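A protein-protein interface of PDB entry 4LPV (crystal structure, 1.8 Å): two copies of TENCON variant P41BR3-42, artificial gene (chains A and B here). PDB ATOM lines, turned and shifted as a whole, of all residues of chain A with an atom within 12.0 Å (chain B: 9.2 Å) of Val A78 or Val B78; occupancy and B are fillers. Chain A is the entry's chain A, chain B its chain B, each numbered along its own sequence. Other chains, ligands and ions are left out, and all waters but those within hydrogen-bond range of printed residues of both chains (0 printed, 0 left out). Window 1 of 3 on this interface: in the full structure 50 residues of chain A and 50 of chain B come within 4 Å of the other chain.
Met A1 touches Lys B80, and with the chains exchanged Lys A80 touches Met B1.
Phe A29 touches Thr B82, and with the chains exchanged Thr A82 touches Phe B29.
Val A75 touches Lys B80, and with the chains exchanged Lys A80 touches Val B75.
Leu A76 touches Val B78, and with the chains exchanged Val A78 touches Leu B76.
Printed residues of chain B within 4 Å of Leu A76: Val B78 (3.5 Å), His B79 (3.4 Å) and Lys B80 (2.7 Å).
Of the printed residues of chain B, Val A77 touches Val B77, Val B78 and His B79.
Of chain B, only Leu B76 (3.4 Å), Val B77 (3.4 Å), Val B78 (2.7 Å) and Lys B80 (3.7 Å) come within 4 Å of Val A78.
Of the printed residues of chain B, His A79 touches Val B75, Leu B76 and Val B77.
Ala B28 touches none of the printed residues of chain A.
Of the printed residues of chain A, Phe B29 touches Thr A82 (3.4 Å).
Of the printed residues of chain A, Val B75 touches His A79 (3.96 Å), Lys A80 (3.3 Å) and Leu A81 (3.8 Å).
Printed residues of chain A within 4 Å of Leu B76: Val A78 (3.4 Å), His A79 (3.6 Å) and Lys A80 (2.8 Å).
Val B77 touches just these residues of chain A: Val A77 (3.5 Å), Val A78 (3.4 Å) and His A79 (3.8 Å).
Of chain A, only Leu A76 (3.5 Å), Val A77 (3.4 Å), Val A78 (2.7 Å) and Lys A80 (3.5 Å) come within 4 Å of Val B78.
Of chain A, only Leu A76 (3.4 Å) and Val A77 (3.5 Å) come within 4 Å of His B79.
Of the printed residues of chain A, Thr B82 touches Leu A2, Pro A3, Phe A29 and Gly A74.
The nearest printed residue of chain B that does not touch His A79 is Val B78 (4.9 Å).
The backbone NH of Val A75 sits at hydrogen-bond distance from the backbone carbonyl oxygen of Ser A31 (2.9 Å).
The backbone carbonyl oxygen (O) of Val B75 lies within hydrogen-bond range of the backbone NH (N) of Asp B30 (2.9 Å).
The side-chain carboxylate (OD1) of Asp B30 lies within hydrogen-bond range of the backbone NH (N) of Val B77, 3.0 Å away.
SD of Met A1 lies close to NZ of Lys B80.
The backbone carbonyl oxygen (O) of Val A78 lies within hydrogen-bond range of the backbone NH (N) of Val B78 (2.7 Å).
O of Leu B76 lies close to O of Val A78 (3.4 Å).
The backbone NH (N) of Lys A80 sits at hydrogen-bond distance from the backbone carbonyl oxygen (O) of Leu B76 (2.8 Å).
The side-chain hydroxyl (OG1) of Thr B82 sits at hydrogen-bond distance from the backbone NH (N) of Gly A74, at 2.9 Å.
The backbone NH of Leu A76 is in hydrogen-bond range of the backbone carbonyl oxygen of Lys B80, at 2.7 Å.
O of Leu A76 lies close to O of Val B78 (3.5 Å).
Of the 17 printed residues of chain A, 13 touch a printed residue of chain B.
Of the 13 printed residues of chain B, 11 touch a printed residue of chain A.
Hydrophobic or aromatic side chains of chain B that line the printed part of chain A: Met B1, Phe B29, Val B75, Val B77, Val B78 and His B79.
Among the printed residues, 29 pairs touch across the chains.
CG2 of Thr B82 touches O of Pro A3, at 3.7 Å.
Lys B80 touches Val A75.
His B79 touches Val A77.
CA of Val B77 touches O of Val A78 (3.4 Å).
CG2 of Val A78 touches CD of Lys B80, 3.7 Å away.
His A79 touches Val B75.
His A79 touches Val B77 (CD2 to CG2, 3.8 Å).
CA of Val B75 touches O of Lys A80, at 3.3 Å.
Lys A80 touches Val B78.
Leu A81 touches Val B75 (CD2 to CG2, 3.8 Å).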
ATOM      1  N   MET A   1      20.907  23.388  17.649  1.00  0.00           N
ATOM      2  CA  MET A   1      21.172  22.777  18.949  1.00  0.00           C
ATOM      3  C   MET A   1      21.779  23.757  19.946  1.00  0.00           C
ATOM      4  O   MET A   1      21.290  23.896  21.066  1.00  0.00           O
ATOM      5  CB  MET A   1      22.087  21.560  18.798  1.00  0.00           C
ATOM      6  CG  MET A   1      21.337  20.241  18.687  1.00  0.00           C
ATOM      7  SD  MET A   1      20.926  19.709  17.015  1.00  0.00           S
ATOM      8  CE  MET A   1      19.756  18.414  17.412  1.00  0.00           C
ATOM      9  N   LEU A   2      22.841  24.439  19.531  1.00  0.00           N
ATOM     10  CA  LEU A   2      23.620  25.280  20.439  1.00  0.00           C
ATOM     11  C   LEU A   2      23.361  26.772  20.212  1.00  0.00           C
ATOM     12  O   LEU A   2      23.015  27.181  19.097  1.00  0.00           O
ATOM     13  CB  LEU A   2      25.109  24.967  20.269  1.00  0.00           C
ATOM     14  CG  LEU A   2      25.371  23.479  20.017  1.00  0.00           C
ATOM     15  CD1 LEU A   2      26.816  23.226  19.564  1.00  0.00           C
ATOM     16  CD2 LEU A   2      24.991  22.642  21.239  1.00  0.00           C
ATOM     17  N   PRO A   3      23.524  27.589  21.274  1.00  0.00           N
ATOM     18  CA  PRO A   3      23.351  29.049  21.183  1.00  0.00           C
ATOM     19  C   PRO A   3      24.232  29.738  20.124  1.00  0.00           C
ATOM     20  O   PRO A   3      25.074  29.109  19.473  1.00  0.00           O
ATOM     21  CB  PRO A   3      23.672  29.547  22.604  1.00  0.00           C
ATOM     22  CG  PRO A   3      24.260  28.366  23.330  1.00  0.00           C
ATOM     23  CD  PRO A   3      23.702  27.149  22.668  1.00  0.00           C
ATOM     24  N   ALA A  27      36.654  28.497  16.605  1.00  0.00           N
ATOM     25  CA  ALA A  27      36.405  27.145  16.113  1.00  0.00           C
ATOM     26  C   ALA A  27      35.055  26.590  16.543  1.00  0.00           C
ATOM     27  O   ALA A  27      34.817  25.397  16.432  1.00  0.00           O
ATOM     28  CB  ALA A  27      37.540  26.202  16.527  1.00  0.00           C
ATOM     29  N   ALA A  28      34.172  27.454  17.037  1.00  0.00           N
ATOM     30  CA  ALA A  28      32.823  27.031  17.392  1.00  0.00           C
ATOM     31  C   ALA A  28      32.037  26.711  16.129  1.00  0.00           C
ATOM     32  O   ALA A  28      31.231  25.782  16.119  1.00  0.00           O
ATOM     33  CB  ALA A  28      32.109  28.101  18.207  1.00  0.00           C
ATOM     34  N   PHE A  29      32.285  27.473  15.064  1.00  0.00           N
ATOM     35  CA  PHE A  29      31.544  27.323  13.814  1.00  0.00           C
ATOM     36  C   PHE A  29      32.458  27.067  12.620  1.00  0.00           C
ATOM     37  O   PHE A  29      33.624  27.444  12.621  1.00  0.00           O
ATOM     38  CB  PHE A  29      30.668  28.556  13.552  1.00  0.00           C
ATOM     39  CG  PHE A  29      29.753  28.893  14.689  1.00  0.00           C
ATOM     40  CD1 PHE A  29      28.666  28.088  14.979  1.00  0.00           C
ATOM     41  CD2 PHE A  29      29.983  30.010  15.479  1.00  0.00           C
ATOM     42  CE1 PHE A  29      27.827  28.392  16.033  1.00  0.00           C
ATOM     43  CE2 PHE A  29      29.145  30.316  16.539  1.00  0.00           C
ATOM     44  CZ  PHE A  29      28.069  29.508  16.815  1.00  0.00           C
ATOM     45  N   ASP A  30      31.909  26.414  11.603  1.00  0.00           N
ATOM     46  CA  ASP A  30      32.646  26.135  10.383  1.00  0.00           C
ATOM     47  C   ASP A  30      32.399  27.259   9.378  1.00  0.00           C
ATOM     48  O   ASP A  30      33.254  27.569   8.540  1.00  0.00           O
ATOM     49  CB  ASP A  30      32.211  24.785   9.791  1.00  0.00           C
ATOM     50  CG  ASP A  30      31.811  23.770  10.864  1.00  0.00           C
ATOM     51  OD1 ASP A  30      31.116  24.165  11.829  1.00  0.00           O
ATOM     52  OD2 ASP A  30      32.194  22.583  10.747  1.00  0.00           O
ATOM     53  N   SER A  31      31.218  27.870   9.477  1.00  0.00           N
ATOM     54  CA  SER A  31      30.806  28.943   8.577  1.00  0.00           C
ATOM     55  C   SER A  31      29.789  29.826   9.291  1.00  0.00           C
ATOM     56  O   SER A  31      29.193  29.403  10.281  1.00  0.00           O
ATOM     57  CB  SER A  31      30.174  28.359   7.298  1.00  0.00           C
ATOM     58  OG  SER A  31      31.077  27.527   6.571  1.00  0.00           O
ATOM     59  N   GLY A  74      25.357  31.118  12.916  1.00  0.00           N
ATOM     60  CA  GLY A  74      26.492  30.224  12.845  1.00  0.00           C
ATOM     61  C   GLY A  74      25.992  28.938  12.235  1.00  0.00           C
ATOM     62  O   GLY A  74      24.842  28.574  12.463  1.00  0.00           O
ATOM     63  N   VAL A  75      26.831  28.277  11.442  1.00  0.00           N
ATOM     64  CA  VAL A  75      26.491  26.966  10.885  1.00  0.00           C
ATOM     65  C   VAL A  75      27.076  25.886  11.786  1.00  0.00           C
ATOM     66  O   VAL A  75      28.291  25.796  11.958  1.00  0.00           O
ATOM     67  CB  VAL A  75      27.026  26.769   9.441  1.00  0.00           C
ATOM     68  CG1 VAL A  75      26.632  25.429   8.908  1.00  0.00           C
ATOM     69  CG2 VAL A  75      26.445  27.834   8.541  1.00  0.00           C
ATOM     70  N   LEU A  76      26.199  25.067  12.351  1.00  0.00           N
ATOM     71  CA  LEU A  76      26.591  23.999  13.251  1.00  0.00           C
ATOM     72  C   LEU A  76      26.464  22.648  12.553  1.00  0.00           C
ATOM     73  O   LEU A  76      25.500  22.401  11.841  1.00  0.00           O
ATOM     74  CB  LEU A  76      25.704  24.032  14.486  1.00  0.00           C
ATOM     75  CG  LEU A  76      26.081  23.034  15.564  1.00  0.00           C
ATOM     76  CD1 LEU A  76      27.449  23.388  16.122  1.00  0.00           C
ATOM     77  CD2 LEU A  76      25.010  23.079  16.617  1.00  0.00           C
ATOM     78  N   VAL A  77      27.452  21.786  12.745  1.00  0.00           N
ATOM     79  CA  VAL A  77      27.412  20.441  12.194  1.00  0.00           C
ATOM     80  C   VAL A  77      26.978  19.483  13.303  1.00  0.00           C
ATOM     81  O   VAL A  77      27.634  19.397  14.331  1.00  0.00           O
ATOM     82  CB  VAL A  77      28.788  20.051  11.600  1.00  0.00           C
ATOM     83  CG1 VAL A  77      28.919  18.551  11.440  1.00  0.00           C
ATOM     84  CG2 VAL A  77      29.007  20.762  10.273  1.00  0.00           C
ATOM     85  N   VAL A  78      25.847  18.810  13.095  1.00  0.00           N
ATOM     86  CA  VAL A  78      25.299  17.856  14.055  1.00  0.00           C
ATOM     87  C   VAL A  78      25.327  16.429  13.487  1.00  0.00           C
ATOM     88  O   VAL A  78      24.995  16.223  12.317  1.00  0.00           O
ATOM     89  CB  VAL A  78      23.830  18.194  14.386  1.00  0.00           C
ATOM     90  CG1 VAL A  78      23.457  17.630  15.729  1.00  0.00           C
ATOM     91  CG2 VAL A  78      23.600  19.698  14.366  1.00  0.00           C
ATOM     92  N   HIS A  79      25.713  15.450  14.304  1.00  0.00           N
ATOM     93  CA  HIS A  79      25.572  14.040  13.918  1.00  0.00           C
ATOM     94  C   HIS A  79      24.254  13.476  14.432  1.00  0.00           C
ATOM     95  O   HIS A  79      23.992  13.478  15.633  1.00  0.00           O
ATOM     96  CB  HIS A  79      26.720  13.180  14.444  1.00  0.00           C
ATOM     97  CG  HIS A  79      28.039  13.463  13.801  1.00  0.00           C
ATOM     98  ND1 HIS A  79      28.920  14.403  14.291  1.00  0.00           N
ATOM     99  CD2 HIS A  79      28.637  12.919  12.715  1.00  0.00           C
ATOM    100  CE1 HIS A  79      30.000  14.430  13.531  1.00  0.00           C
ATOM    101  NE2 HIS A  79      29.851  13.542  12.563  1.00  0.00           N
ATOM    102  N   LYS A  80      23.427  12.991  13.518  1.00  0.00           N
ATOM    103  CA  LYS A  80      22.175  12.365  13.887  1.00  0.00           C
ATOM    104  C   LYS A  80      22.223  10.860  13.644  1.00  0.00           C
ATOM    105  O   LYS A  80      22.945  10.382  12.765  1.00  0.00           O
ATOM    106  CB  LYS A  80      21.011  12.998  13.124  1.00  0.00           C
ATOM    107  CG  LYS A  80      20.824  14.467  13.451  1.00  0.00           C
ATOM    108  CD  LYS A  80      19.384  14.887  13.296  1.00  0.00           C
ATOM    109  CE  LYS A  80      19.100  16.020  14.245  1.00  0.00           C
ATOM    110  NZ  LYS A  80      19.780  15.767  15.542  1.00  0.00           N
ATOM    111  N   LEU A  81      21.458  10.129  14.449  1.00  0.00           N
ATOM    112  CA  LEU A  81      21.295   8.692  14.289  1.00  0.00           C
ATOM    113  C   LEU A  81      19.864   8.348  13.856  1.00  0.00           C
ATOM    114  O   LEU A  81      18.896   9.011  14.244  1.00  0.00           O
ATOM    115  CB  LEU A  81      21.615   7.966  15.599  1.00  0.00           C
ATOM    116  CG  LEU A  81      22.976   8.129  16.272  1.00  0.00           C
ATOM    117  CD1 LEU A  81      22.998   7.273  17.518  1.00  0.00           C
ATOM    118  CD2 LEU A  81      24.095   7.729  15.330  1.00  0.00           C
ATOM    119  N   THR A  82      19.734   7.304  13.046  1.00  0.00           N
ATOM    120  CA  THR A  82      18.424   6.753  12.755  1.00  0.00           C
ATOM    121  C   THR A  82      18.035   5.871  13.929  1.00  0.00           C
ATOM    122  O   THR A  82      18.841   5.652  14.830  1.00  0.00           O
ATOM    123  CB  THR A  82      18.411   5.892  11.456  1.00  0.00           C
ATOM    124  OG1 THR A  82      19.279   4.758  11.603  1.00  0.00           O
ATOM    125  CG2 THR A  82      18.843   6.698  10.245  1.00  0.00           C
ATOM    126  N   MET B   1      16.301  11.565  11.749  1.00  0.00           N
ATOM    127  CA  MET B   1      15.248  12.032  10.850  1.00  0.00           C
ATOM    128  C   MET B   1      14.936  10.952   9.824  1.00  0.00           C
ATOM    129  O   MET B   1      13.874  10.324   9.858  1.00  0.00           O
ATOM    130  CB  MET B   1      15.677  13.318  10.118  1.00  0.00           C
ATOM    131  CG  MET B   1      16.070  14.491  11.017  1.00  0.00           C
ATOM    132  SD  MET B   1      16.917  15.828  10.128  1.00  0.00           S
ATOM    133  CE  MET B   1      17.207  16.981  11.476  1.00  0.00           C
ATOM    134  N   LEU B   2      15.882  10.759   8.908  1.00  0.00           N
ATOM    135  CA  LEU B   2      15.770   9.792   7.822  1.00  0.00           C
ATOM    136  C   LEU B   2      15.550   8.375   8.363  1.00  0.00           C
ATOM    137  O   LEU B   2      16.049   8.038   9.442  1.00  0.00           O
ATOM    138  CB  LEU B   2      17.034   9.841   6.955  1.00  0.00           C
ATOM    139  CG  LEU B   2      17.565  11.217   6.525  1.00  0.00           C
ATOM    140  CD1 LEU B   2      18.870  11.072   5.738  1.00  0.00           C
ATOM    141  CD2 LEU B   2      16.526  11.978   5.714  1.00  0.00           C
ATOM    142  N   ALA B  28      22.405   9.000   1.310  1.00  0.00           N
ATOM    143  CA  ALA B  28      21.618   9.252   2.531  1.00  0.00           C
ATOM    144  C   ALA B  28      22.463   9.518   3.794  1.00  0.00           C
ATOM    145  O   ALA B  28      22.246  10.509   4.492  1.00  0.00           O
ATOM    146  CB  ALA B  28      20.643   8.100   2.780  1.00  0.00           C
ATOM    147  N   PHE B  29      23.421   8.635   4.086  1.00  0.00           N
ATOM    148  CA  PHE B  29      24.204   8.727   5.327  1.00  0.00           C
ATOM    149  C   PHE B  29      25.702   8.943   5.102  1.00  0.00           C
ATOM    150  O   PHE B  29      26.263   8.477   4.118  1.00  0.00           O
ATOM    151  CB  PHE B  29      23.958   7.486   6.202  1.00  0.00           C
ATOM    152  CG  PHE B  29      22.501   7.227   6.466  1.00  0.00           C
ATOM    153  CD1 PHE B  29      21.783   8.066   7.297  1.00  0.00           C
ATOM    154  CD2 PHE B  29      21.844   6.167   5.849  1.00  0.00           C
ATOM    155  CE1 PHE B  29      20.437   7.857   7.529  1.00  0.00           C
ATOM    156  CE2 PHE B  29      20.487   5.942   6.076  1.00  0.00           C
ATOM    157  CZ  PHE B  29      19.784   6.792   6.919  1.00  0.00           C
ATOM    158  N   ASP B  30      26.340   9.651   6.024  1.00  0.00           N
ATOM    159  CA  ASP B  30      27.769   9.912   5.942  1.00  0.00           C
ATOM    160  C   ASP B  30      28.544   8.743   6.514  1.00  0.00           C
ATOM    161  O   ASP B  30      29.689   8.518   6.151  1.00  0.00           O
ATOM    162  CB  ASP B  30      28.127  11.196   6.703  1.00  0.00           C
ATOM    163  CG  ASP B  30      27.450  12.431   6.118  1.00  0.00           C
ATOM    164  OD1 ASP B  30      26.245  12.615   6.383  1.00  0.00           O
ATOM    165  OD2 ASP B  30      28.117  13.217   5.404  1.00  0.00           O
ATOM    166  N   VAL B  75      24.147   7.191  10.112  1.00  0.00           N
ATOM    167  CA  VAL B  75      24.613   8.440  10.709  1.00  0.00           C
ATOM    168  C   VAL B  75      24.516   9.565   9.669  1.00  0.00           C
ATOM    169  O   VAL B  75      25.076   9.477   8.573  1.00  0.00           O
ATOM    170  CB  VAL B  75      26.075   8.331  11.255  1.00  0.00           C
ATOM    171  CG1 VAL B  75      26.546   9.661  11.880  1.00  0.00           C
ATOM    172  CG2 VAL B  75      26.202   7.192  12.250  1.00  0.00           C
ATOM    173  N   LEU B  76      23.782  10.616  10.016  1.00  0.00           N
ATOM    174  CA  LEU B  76      23.597  11.752   9.125  1.00  0.00           C
ATOM    175  C   LEU B  76      24.208  13.014   9.719  1.00  0.00           C
ATOM    176  O   LEU B  76      23.810  13.452  10.798  1.00  0.00           O
ATOM    177  CB  LEU B  76      22.112  11.979   8.865  1.00  0.00           C
ATOM    178  CG  LEU B  76      21.801  13.187   7.985  1.00  0.00           C
ATOM    179  CD1 LEU B  76      22.318  12.950   6.563  1.00  0.00           C
ATOM    180  CD2 LEU B  76      20.301  13.494   8.003  1.00  0.00           C
ATOM    181  N   VAL B  77      25.189  13.574   9.018  1.00  0.00           N
ATOM    182  CA  VAL B  77      25.743  14.889   9.335  1.00  0.00           C
ATOM    183  C   VAL B  77      24.750  15.961   8.865  1.00  0.00           C
ATOM    184  O   VAL B  77      24.514  16.140   7.659  1.00  0.00           O
ATOM    185  CB  VAL B  77      27.129  15.111   8.657  1.00  0.00           C
ATOM    186  CG1 VAL B  77      27.599  16.542   8.830  1.00  0.00           C
ATOM    187  CG2 VAL B  77      28.171  14.123   9.194  1.00  0.00           C
ATOM    188  N   VAL B  78      24.145  16.634   9.839  1.00  0.00           N
ATOM    189  CA  VAL B  78      23.174  17.685   9.590  1.00  0.00           C
ATOM    190  C   VAL B  78      23.891  19.020   9.755  1.00  0.00           C
ATOM    191  O   VAL B  78      24.666  19.202  10.696  1.00  0.00           O
ATOM    192  CB  VAL B  78      21.974  17.567  10.570  1.00  0.00           C
ATOM    193  CG1 VAL B  78      20.956  18.639  10.284  1.00  0.00           C
ATOM    194  CG2 VAL B  78      21.323  16.206  10.432  1.00  0.00           C
ATOM    195  N   HIS B  79      23.671  19.935   8.819  1.00  0.00           N
ATOM    196  CA  HIS B  79      24.262  21.261   8.904  1.00  0.00           C
ATOM    197  C   HIS B  79      23.161  22.233   9.305  1.00  0.00           C
ATOM    198  O   HIS B  79      22.355  22.635   8.472  1.00  0.00           O
ATOM    199  CB  HIS B  79      24.891  21.651   7.562  1.00  0.00           C
ATOM    200  CG  HIS B  79      25.841  20.627   7.016  1.00  0.00           C
ATOM    201  ND1 HIS B  79      27.190  20.639   7.294  1.00  0.00           N
ATOM    202  CD2 HIS B  79      25.634  19.554   6.215  1.00  0.00           C
ATOM    203  CE1 HIS B  79      27.775  19.619   6.689  1.00  0.00           C
ATOM    204  NE2 HIS B  79      26.851  18.948   6.025  1.00  0.00           N
ATOM    205  N   LYS B  80      23.122  22.582  10.591  1.00  0.00           N
ATOM    206  CA  LYS B  80      22.058  23.406  11.161  1.00  0.00           C
ATOM    207  C   LYS B  80      22.444  24.865  11.406  1.00  0.00           C
ATOM    208  O   LYS B  80      23.604  25.184  11.658  1.00  0.00           O
ATOM    209  CB  LYS B  80      21.559  22.802  12.487  1.00  0.00           C
ATOM    210  CG  LYS B  80      20.824  21.476  12.332  1.00  0.00           C
ATOM    211  CD  LYS B  80      20.225  21.010  13.645  1.00  0.00           C
ATOM    212  CE  LYS B  80      19.755  19.566  13.571  1.00  0.00           C
ATOM    213  NZ  LYS B  80      18.699  19.309  14.588  1.00  0.00           N
ATOM    214  N   LEU B  81      21.440  25.736  11.363  1.00  0.00           N
ATOM    215  CA  LEU B  81      21.629  27.159  11.633  1.00  0.00           C
ATOM    216  C   LEU B  81      21.249  27.488  13.080  1.00  0.00           C
ATOM    217  O   LEU B  81      20.286  26.947  13.613  1.00  0.00           O
ATOM    218  CB  LEU B  81      20.781  27.985  10.669  1.00  0.00           C
ATOM    219  CG  LEU B  81      20.928  27.732   9.166  1.00  0.00           C
ATOM    220  CD1 LEU B  81      19.975  28.624   8.370  1.00  0.00           C
ATOM    221  CD2 LEU B  81      22.383  27.918   8.713  1.00  0.00           C
ATOM    222  N   THR B  82      22.012  28.370  13.721  1.00  0.00           N
ATOM    223  CA  THR B  82      21.662  28.840  15.059  1.00  0.00           C
ATOM    224  C   THR B  82      20.422  29.746  14.988  1.00  0.00           C
ATOM    225  O   THR B  82      19.995  30.134  13.898  1.00  0.00           O
ATOM    226  CB  THR B  82      22.842  29.621  15.727  1.00  0.00           C
ATOM    227  OG1 THR B  82      23.255  30.694  14.874  1.00  0.00           O
ATOM    228  CG2 THR B  82      24.042  28.708  15.987  1.00  0.00           C
